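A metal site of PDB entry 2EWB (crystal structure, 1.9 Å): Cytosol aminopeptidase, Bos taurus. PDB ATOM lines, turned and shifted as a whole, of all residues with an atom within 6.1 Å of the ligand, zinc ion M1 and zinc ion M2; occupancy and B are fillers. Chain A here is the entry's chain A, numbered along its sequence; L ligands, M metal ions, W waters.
Four residues have an atom within 4 Å of zinc ion M1: Lys 250, Asp 255, Asp 273 and Glu 334.
Zinc ion M2 is bound by the side-chain carboxylate (OD1) of Asp 332, the side-chain carboxylate (OE1) of Glu 334, the side-chain carboxylate (OD2) of Asp 255, the backbone carbonyl oxygen (O) of Asp 332 and a sulfur (S2) of the ligand.
NZ of Lys 262 sits at hydrogen-bond distance from O3 of the ligand, 2.8 Å away.
Zinc ion M1 is bound by the side-chain carboxylate (OD2) of Asp 273 (1.9 Å), the side-chain carboxylate (OE2) of Glu 334 (2.0 Å), the side-chain amino group (NZ) of Lys 250 (2.1 Å) and a sulfur (S2) of the ligand (2.3 Å). Zinc ion M1 has four donor atoms within binding distance. Slightly farther from zinc ion M1 lies the side-chain carboxylate (OD2) of Asp 255 (2.8 Å).
Met 270 touches the ligand (CE to S2, 3.8 Å). Asn 330 touches the ligand (OD1 to C9, 3.7 Å). Ala 333 touches the ligand. Arg 336 touches the ligand (NH2 to C11, 3.98 Å). Leu 360 touches the ligand. Thr 361 touches the ligand (CA to C12, 3.6 Å). N of Gly 362 touches C12 of the ligand (3.4 Å). Ile 421 touches the ligand.
The side-chain hydroxyl (OG1) of Thr 359 sits at hydrogen-bond distance from the side-chain carboxylate (OD1) of Asp 273 (2.6 Å). The backbone NH (N) of Ile 252 lies within hydrogen-bond range of the backbone carbonyl oxygen (O) of Asp 273, 3.3 Å away. The side-chain amide oxygen (OD1) of Asn 330 lies within hydrogen-bond range of the backbone NH (N) of Asp 332, 2.6 Å away. The backbone NH (N) of Asp 332 lies within hydrogen-bond range of the backbone carbonyl oxygen (O) of Gly 257 (3.3 Å). The side-chain carboxylate (OE1) of Glu 334 lies close to the side-chain amide nitrogen (ND2) of Asn 305 (3.3 Å). NZ of Lys 262 sits close to OD2 of Asp 255 (3.8 Å). N of Asp 255 sits at hydrogen-bond distance from O of Met 270, at 3.5 Å. NH1 of Arg 336 lies within hydrogen-bond range of O of Asn 420, 2.9 Å away.
Water W6 bridges O1 of the ligand (2.7 Å) and ND2 of Asn 330 (2.9 Å). Water W3 lies within hydrogen-bond range of the backbone NH (N) of Gly 362 (2.7 Å) and an oxygen (O2) of the ligand (2.8 Å).
NZ of Lys 262 touches zinc ion M2, 3.9 Å away. Four residues have an atom within 4 Å of zinc ion M2: Asp 255, Lys 262, Asp 332 and Glu 334. The nearest printed residue that does not touch zinc ion M2 is Ala 333 (4.2 Å).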
ATOM      1  N   LYS A 250     -21.472   7.154  35.676  1.00  0.00           N
ATOM      2  CA  LYS A 250     -20.961   8.003  34.608  1.00  0.00           C
ATOM      3  C   LYS A 250     -21.689   9.335  34.708  1.00  0.00           C
ATOM      4  O   LYS A 250     -22.913   9.390  34.585  1.00  0.00           O
ATOM      5  CB  LYS A 250     -21.236   7.357  33.250  1.00  0.00           C
ATOM      6  CG  LYS A 250     -20.989   8.275  32.054  1.00  0.00           C
ATOM      7  CD  LYS A 250     -21.388   7.587  30.734  1.00  0.00           C
ATOM      8  CE  LYS A 250     -21.242   8.544  29.559  1.00  0.00           C
ATOM      9  NZ  LYS A 250     -21.619   7.909  28.264  1.00  0.00           N
ATOM     10  N   ILE A 252     -21.498  12.370  32.741  1.00  0.00           N
ATOM     11  CA  ILE A 252     -21.265  13.317  31.652  1.00  0.00           C
ATOM     12  C   ILE A 252     -22.520  14.200  31.628  1.00  0.00           C
ATOM     13  O   ILE A 252     -23.569  13.770  31.142  1.00  0.00           O
ATOM     14  CB  ILE A 252     -21.084  12.594  30.306  1.00  0.00           C
ATOM     15  CG1 ILE A 252     -19.815  11.730  30.349  1.00  0.00           C
ATOM     16  CG2 ILE A 252     -20.990  13.608  29.175  1.00  0.00           C
ATOM     17  CD1 ILE A 252     -18.522  12.529  30.473  1.00  0.00           C
ATOM     18  N   ASP A 255     -23.034  15.493  26.647  1.00  0.00           N
ATOM     19  CA  ASP A 255     -22.132  14.852  25.719  1.00  0.00           C
ATOM     20  C   ASP A 255     -22.411  15.249  24.279  1.00  0.00           C
ATOM     21  O   ASP A 255     -23.423  14.857  23.697  1.00  0.00           O
ATOM     22  CB  ASP A 255     -22.235  13.343  25.875  1.00  0.00           C
ATOM     23  CG  ASP A 255     -21.214  12.602  25.051  1.00  0.00           C
ATOM     24  OD1 ASP A 255     -20.232  13.234  24.620  1.00  0.00           O
ATOM     25  OD2 ASP A 255     -21.387  11.392  24.858  1.00  0.00           O
ATOM     26  N   GLY A 257     -20.155  14.567  22.141  1.00  0.00           N
ATOM     27  CA  GLY A 257     -19.332  13.591  21.453  1.00  0.00           C
ATOM     28  C   GLY A 257     -17.891  14.086  21.389  1.00  0.00           C
ATOM     29  O   GLY A 257     -16.956  13.308  21.228  1.00  0.00           O
ATOM     30  N   LYS A 262     -21.249  14.255  17.770  1.00  0.00           N
ATOM     31  CA  LYS A 262     -22.505  13.562  17.516  1.00  0.00           C
ATOM     32  C   LYS A 262     -23.325  14.282  16.455  1.00  0.00           C
ATOM     33  O   LYS A 262     -23.086  15.457  16.162  1.00  0.00           O
ATOM     34  CB  LYS A 262     -23.351  13.490  18.782  1.00  0.00           C
ATOM     35  CG  LYS A 262     -22.772  12.623  19.878  1.00  0.00           C
ATOM     36  CD  LYS A 262     -23.627  12.732  21.131  1.00  0.00           C
ATOM     37  CE  LYS A 262     -23.131  11.777  22.201  1.00  0.00           C
ATOM     38  NZ  LYS A 262     -23.239  10.378  21.735  1.00  0.00           N
ATOM     39  N   MET A 270     -28.651  14.056  25.347  1.00  0.00           N
ATOM     40  CA  MET A 270     -27.359  13.783  25.962  1.00  0.00           C
ATOM     41  C   MET A 270     -27.161  14.574  27.250  1.00  0.00           C
ATOM     42  O   MET A 270     -26.113  14.466  27.898  1.00  0.00           O
ATOM     43  CB  MET A 270     -26.228  14.036  24.974  1.00  0.00           C
ATOM     44  CG  MET A 270     -26.224  13.085  23.789  1.00  0.00           C
ATOM     45  SD  MET A 270     -26.468  11.352  24.265  1.00  0.00           S
ATOM     46  CE  MET A 270     -25.035  11.057  25.223  1.00  0.00           C
ATOM     47  N   ASP A 273     -26.714  12.128  29.881  1.00  0.00           N
ATOM     48  CA  ASP A 273     -25.575  11.227  29.802  1.00  0.00           C
ATOM     49  C   ASP A 273     -24.900  11.121  31.159  1.00  0.00           C
ATOM     50  O   ASP A 273     -23.823  10.543  31.299  1.00  0.00           O
ATOM     51  CB  ASP A 273     -24.593  11.719  28.737  1.00  0.00           C
ATOM     52  CG  ASP A 273     -23.715  10.605  28.191  1.00  0.00           C
ATOM     53  OD1 ASP A 273     -24.177   9.442  28.147  1.00  0.00           O
ATOM     54  OD2 ASP A 273     -22.571  10.888  27.778  1.00  0.00           O
ATOM     55  N   ASN A 305     -18.490  16.765  27.754  1.00  0.00           N
ATOM     56  CA  ASN A 305     -17.635  16.281  26.676  1.00  0.00           C
ATOM     57  C   ASN A 305     -17.929  17.243  25.548  1.00  0.00           C
ATOM     58  O   ASN A 305     -18.950  17.135  24.870  1.00  0.00           O
ATOM     59  CB  ASN A 305     -17.978  14.846  26.291  1.00  0.00           C
ATOM     60  CG  ASN A 305     -16.987  14.254  25.313  1.00  0.00           C
ATOM     61  OD1 ASN A 305     -15.821  14.663  25.264  1.00  0.00           O
ATOM     62  ND2 ASN A 305     -17.427  13.276  24.540  1.00  0.00           N
ATOM     63  N   ASN A 330     -12.115   7.215  19.588  1.00  0.00           N
ATOM     64  CA  ASN A 330     -13.372   7.916  19.412  1.00  0.00           C
ATOM     65  C   ASN A 330     -13.661   8.684  20.699  1.00  0.00           C
ATOM     66  O   ASN A 330     -13.900   8.092  21.745  1.00  0.00           O
ATOM     67  CB  ASN A 330     -14.493   6.934  19.105  1.00  0.00           C
ATOM     68  CG  ASN A 330     -15.787   7.631  18.755  1.00  0.00           C
ATOM     69  OD1 ASN A 330     -16.249   8.504  19.485  1.00  0.00           O
ATOM     70  ND2 ASN A 330     -16.403   7.233  17.641  1.00  0.00           N
ATOM     71  N   THR A 331     -13.630  10.005  20.605  1.00  0.00           N
ATOM     72  CA  THR A 331     -13.850  10.849  21.768  1.00  0.00           C
ATOM     73  C   THR A 331     -15.274  10.794  22.306  1.00  0.00           C
ATOM     74  O   THR A 331     -15.551  11.330  23.369  1.00  0.00           O
ATOM     75  CB  THR A 331     -13.498  12.315  21.473  1.00  0.00           C
ATOM     76  OG1 THR A 331     -14.456  12.858  20.541  1.00  0.00           O
ATOM     77  CG2 THR A 331     -12.101  12.408  20.856  1.00  0.00           C
ATOM     78  N   ASP A 332     -16.167  10.150  21.552  1.00  0.00           N
ATOM     79  CA  ASP A 332     -17.552  10.046  21.983  1.00  0.00           C
ATOM     80  C   ASP A 332     -17.747   8.784  22.830  1.00  0.00           C
ATOM     81  O   ASP A 332     -18.845   8.509  23.312  1.00  0.00           O
ATOM     82  CB  ASP A 332     -18.490  10.039  20.769  1.00  0.00           C
ATOM     83  CG  ASP A 332     -19.943  10.287  21.143  1.00  0.00           C
ATOM     84  OD1 ASP A 332     -20.204  10.676  22.306  1.00  0.00           O
ATOM     85  OD2 ASP A 332     -20.813  10.105  20.270  1.00  0.00           O
ATOM     86  N   ALA A 333     -16.677   8.009  22.993  1.00  0.00           N
ATOM     87  CA  ALA A 333     -16.721   6.828  23.842  1.00  0.00           C
ATOM     88  C   ALA A 333     -16.001   7.338  25.102  1.00  0.00           C
ATOM     89  O   ALA A 333     -15.023   6.758  25.552  1.00  0.00           O
ATOM     90  CB  ALA A 333     -15.935   5.686  23.215  1.00  0.00           C
ATOM     91  N   GLU A 334     -16.515   8.436  25.634  1.00  0.00           N
ATOM     92  CA  GLU A 334     -15.914   9.093  26.792  1.00  0.00           C
ATOM     93  C   GLU A 334     -16.344   8.563  28.152  1.00  0.00           C
ATOM     94  O   GLU A 334     -15.632   8.731  29.138  1.00  0.00           O
ATOM     95  CB  GLU A 334     -16.169  10.606  26.735  1.00  0.00           C
ATOM     96  CG  GLU A 334     -17.530  11.067  27.291  1.00  0.00           C
ATOM     97  CD  GLU A 334     -18.739  10.481  26.569  1.00  0.00           C
ATOM     98  OE1 GLU A 334     -18.684  10.349  25.337  1.00  0.00           O
ATOM     99  OE2 GLU A 334     -19.742  10.171  27.252  1.00  0.00           O
ATOM    100  N   GLY A 335     -17.515   7.948  28.201  1.00  0.00           N
ATOM    101  CA  GLY A 335     -18.006   7.422  29.460  1.00  0.00           C
ATOM    102  C   GLY A 335     -17.093   6.360  30.032  1.00  0.00           C
ATOM    103  O   GLY A 335     -16.828   6.340  31.242  1.00  0.00           O
ATOM    104  N   ARG A 336     -16.578   5.478  29.179  1.00  0.00           N
ATOM    105  CA  ARG A 336     -15.693   4.437  29.656  1.00  0.00           C
ATOM    106  C   ARG A 336     -14.359   5.040  30.098  1.00  0.00           C
ATOM    107  O   ARG A 336     -13.676   4.489  30.954  1.00  0.00           O
ATOM    108  CB  ARG A 336     -15.486   3.365  28.582  1.00  0.00           C
ATOM    109  CG  ARG A 336     -14.751   3.822  27.338  1.00  0.00           C
ATOM    110  CD  ARG A 336     -14.993   2.821  26.207  1.00  0.00           C
ATOM    111  NE  ARG A 336     -16.335   2.981  25.643  1.00  0.00           N
ATOM    112  CZ  ARG A 336     -16.841   2.219  24.676  1.00  0.00           C
ATOM    113  NH1 ARG A 336     -16.137   1.217  24.179  1.00  0.00           N
ATOM    114  NH2 ARG A 336     -18.055   2.476  24.208  1.00  0.00           N
ATOM    115  N   THR A 359     -24.981   5.470  31.044  1.00  0.00           N
ATOM    116  CA  THR A 359     -25.736   5.534  29.801  1.00  0.00           C
ATOM    117  C   THR A 359     -24.562   5.345  28.850  1.00  0.00           C
ATOM    118  O   THR A 359     -24.158   6.268  28.133  1.00  0.00           O
ATOM    119  CB  THR A 359     -26.345   6.917  29.625  1.00  0.00           C
ATOM    120  OG1 THR A 359     -25.358   7.905  29.930  1.00  0.00           O
ATOM    121  CG2 THR A 359     -27.541   7.099  30.551  1.00  0.00           C
ATOM    122  N   LEU A 360     -24.018   4.141  28.854  1.00  0.00           N
ATOM    123  CA  LEU A 360     -22.818   3.845  28.097  1.00  0.00           C
ATOM    124  C   LEU A 360     -22.839   3.611  26.595  1.00  0.00           C
ATOM    125  O   LEU A 360     -21.959   4.099  25.907  1.00  0.00           O
ATOM    126  CB  LEU A 360     -22.088   2.678  28.762  1.00  0.00           C
ATOM    127  CG  LEU A 360     -20.573   2.623  28.533  1.00  0.00           C
ATOM    128  CD1 LEU A 360     -19.917   3.852  29.173  1.00  0.00           C
ATOM    129  CD2 LEU A 360     -20.020   1.352  29.145  1.00  0.00           C
ATOM    130  N   THR A 361     -23.802   2.869  26.082  1.00  0.00           N
ATOM    131  CA  THR A 361     -23.763   2.605  24.644  1.00  0.00           C
ATOM    132  C   THR A 361     -25.100   2.612  23.942  1.00  0.00           C
ATOM    133  O   THR A 361     -26.124   2.210  24.496  1.00  0.00           O
ATOM    134  CB  THR A 361     -23.114   1.240  24.352  1.00  0.00           C
ATOM    135  OG1 THR A 361     -23.948   0.191  24.874  1.00  0.00           O
ATOM    136  CG2 THR A 361     -21.732   1.145  24.995  1.00  0.00           C
ATOM    137  N   GLY A 362     -25.088   3.080  22.694  1.00  0.00           N
ATOM    138  CA  GLY A 362     -26.302   3.088  21.902  1.00  0.00           C
ATOM    139  C   GLY A 362     -26.560   1.627  21.575  1.00  0.00           C
ATOM    140  O   GLY A 362     -27.683   1.217  21.327  1.00  0.00           O
ATOM    141  N   ALA A 363     -25.489   0.842  21.591  1.00  0.00           N
ATOM    142  CA  ALA A 363     -25.599  -0.590  21.300  1.00  0.00           C
ATOM    143  C   ALA A 363     -26.521  -1.260  22.306  1.00  0.00           C
ATOM    144  O   ALA A 363     -27.252  -2.186  21.959  1.00  0.00           O
ATOM    145  CB  ALA A 363     -24.220  -1.239  21.337  1.00  0.00           C
ATOM    146  N   ASN A 420     -10.319   2.584  23.343  1.00  0.00           N
ATOM    147  CA  ASN A 420     -11.620   2.926  23.908  1.00  0.00           C
ATOM    148  C   ASN A 420     -12.816   2.562  23.024  1.00  0.00           C
ATOM    149  O   ASN A 420     -13.956   2.893  23.358  1.00  0.00           O
ATOM    150  CB  ASN A 420     -11.652   4.400  24.355  1.00  0.00           C
ATOM    151  CG  ASN A 420     -12.010   5.361  23.242  1.00  0.00           C
ATOM    152  OD1 ASN A 420     -11.594   5.199  22.092  1.00  0.00           O
ATOM    153  ND2 ASN A 420     -12.763   6.397  23.586  1.00  0.00           N
ATOM    154  N   ILE A 421     -12.547   1.894  21.906  1.00  0.00           N
ATOM    155  CA  ILE A 421     -13.606   1.407  21.026  1.00  0.00           C
ATOM    156  C   ILE A 421     -13.119   0.078  20.455  1.00  0.00           C
ATOM    157  O   ILE A 421     -11.933  -0.098  20.188  1.00  0.00           O
ATOM    158  CB  ILE A 421     -13.932   2.373  19.855  1.00  0.00           C
ATOM    159  CG1 ILE A 421     -12.719   2.541  18.937  1.00  0.00           C
ATOM    160  CG2 ILE A 421     -14.422   3.686  20.397  1.00  0.00           C
ATOM    161  CD1 ILE A 421     -13.045   3.264  17.640  1.00  0.00           C
ATOM    162  N   GLY A 422     -14.040  -0.875  20.288  1.00  0.00           N
ATOM    163  CA  GLY A 422     -13.672  -2.171  19.770  1.00  0.00           C
ATOM    164  C   GLY A 422     -13.179  -2.101  18.339  1.00  0.00           C
ATOM    165  O   GLY A 422     -13.438  -1.122  17.640  1.00  0.00           O
ATOM    166  N   TYR A 424     -14.170  -3.966  16.028  1.00  0.00           N
ATOM    167  CA  TYR A 424     -15.335  -4.246  15.198  1.00  0.00           C
ATOM    168  C   TYR A 424     -16.483  -3.413  15.773  1.00  0.00           C
ATOM    169  O   TYR A 424     -16.434  -2.984  16.924  1.00  0.00           O
ATOM    170  CB  TYR A 424     -15.689  -5.738  15.237  1.00  0.00           C
ATOM    171  CG  TYR A 424     -14.555  -6.673  14.866  1.00  0.00           C
ATOM    172  CD1 TYR A 424     -13.777  -6.453  13.726  1.00  0.00           C
ATOM    173  CD2 TYR A 424     -14.260  -7.777  15.660  1.00  0.00           C
ATOM    174  CE1 TYR A 424     -12.743  -7.326  13.383  1.00  0.00           C
ATOM    175  CE2 TYR A 424     -13.228  -8.657  15.324  1.00  0.00           C
ATOM    176  CZ  TYR A 424     -12.465  -8.422  14.181  1.00  0.00           C
ATOM    177  OH  TYR A 424     -11.440  -9.275  13.856  1.00  0.00           O
ATOM    178  N   ARG A 425     -17.513  -3.177  14.972  1.00  0.00           N
ATOM    179  CA  ARG A 425     -18.643  -2.377  15.424  1.00  0.00           C
ATOM    180  C   ARG A 425     -19.716  -3.213  16.119  1.00  0.00           C
ATOM    181  O   ARG A 425     -20.689  -2.679  16.637  1.00  0.00           O
ATOM    182  CB  ARG A 425     -19.252  -1.620  14.237  1.00  0.00           C
ATOM    183  N   ALA A 451     -28.228   2.979  29.031  1.00  0.00           N
ATOM    184  CA  ALA A 451     -28.495   3.818  27.876  1.00  0.00           C
ATOM    185  C   ALA A 451     -29.881   3.561  27.278  1.00  0.00           C
ATOM    186  O   ALA A 451     -30.564   4.493  26.854  1.00  0.00           O
ATOM    187  CB  ALA A 451     -27.418   3.609  26.810  1.00  0.00           C
HETATM  188  C1  LIG L   1     -17.546   2.875  18.550  1.00  0.00           C
HETATM  189  C2  LIG L   1     -18.832   3.427  18.477  1.00  0.00           C
HETATM  190  C3  LIG L   1     -19.289   3.934  17.234  1.00  0.00           C
HETATM  191  C4  LIG L   1     -18.467   3.886  16.086  1.00  0.00           C
HETATM  192  C5  LIG L   1     -17.173   3.323  16.164  1.00  0.00           C
HETATM  193  C6  LIG L   1     -16.711   2.806  17.399  1.00  0.00           C
HETATM  194  C7  LIG L   1     -20.558   6.748  20.263  1.00  0.00           C
HETATM  195  C8  LIG L   1     -21.457   6.353  19.067  1.00  0.00           C
HETATM  196  C9  LIG L   1     -19.111   6.273  20.129  1.00  0.00           C
HETATM  197  C10 LIG L   1     -19.126   4.920  20.839  1.00  0.00           C
HETATM  198  C11 LIG L   1     -19.903   5.281  22.075  1.00  0.00           C
HETATM  199  C12 LIG L   1     -23.946   6.120  23.771  1.00  0.00           C
HETATM  200  C13 LIG L   1     -22.411   6.183  23.585  1.00  0.00           C
HETATM  201  C14 LIG L   1     -22.017   6.743  22.206  1.00  0.00           C
HETATM  202  C15 LIG L   1     -21.778   6.951  24.754  1.00  0.00           C
HETATM  203  O1  LIG L   1     -21.224   6.826  17.953  1.00  0.00           O
HETATM  204  O2  LIG L   1     -22.400   5.578  19.264  1.00  0.00           O
HETATM  205  O3  LIG L   1     -22.654   7.688  21.720  1.00  0.00           O
HETATM  206  N1  LIG L   1     -20.975   6.169  21.552  1.00  0.00           N
HETATM  207  S1  LIG L   1     -19.876   3.513  19.953  1.00  0.00           S
HETATM  208  S2  LIG L   1     -22.023   8.720  24.755  1.00  0.00           S
HETATM  209 ZN    ZN M   1     -21.598   9.443  26.902  1.00  0.00          ZN
HETATM  210 ZN    ZN M   2     -20.211   9.954  24.128  1.00  0.00          ZN
HETATM  211  O   HOH W   1     -20.308   1.009  15.626  1.00  0.00           O
HETATM  212  O   HOH W   2     -17.736  -0.269  19.256  1.00  0.00           O
HETATM  213  O   HOH W   3     -22.890   3.793  21.334  1.00  0.00           O
HETATM  214  O   HOH W   4     -17.170   5.916  13.599  1.00  0.00           O
HETATM  215  O   HOH W   5     -22.023   1.150  21.023  1.00  0.00           O
HETATM  216  O   HOH W   6     -19.099   8.122  16.912  1.00  0.00           O
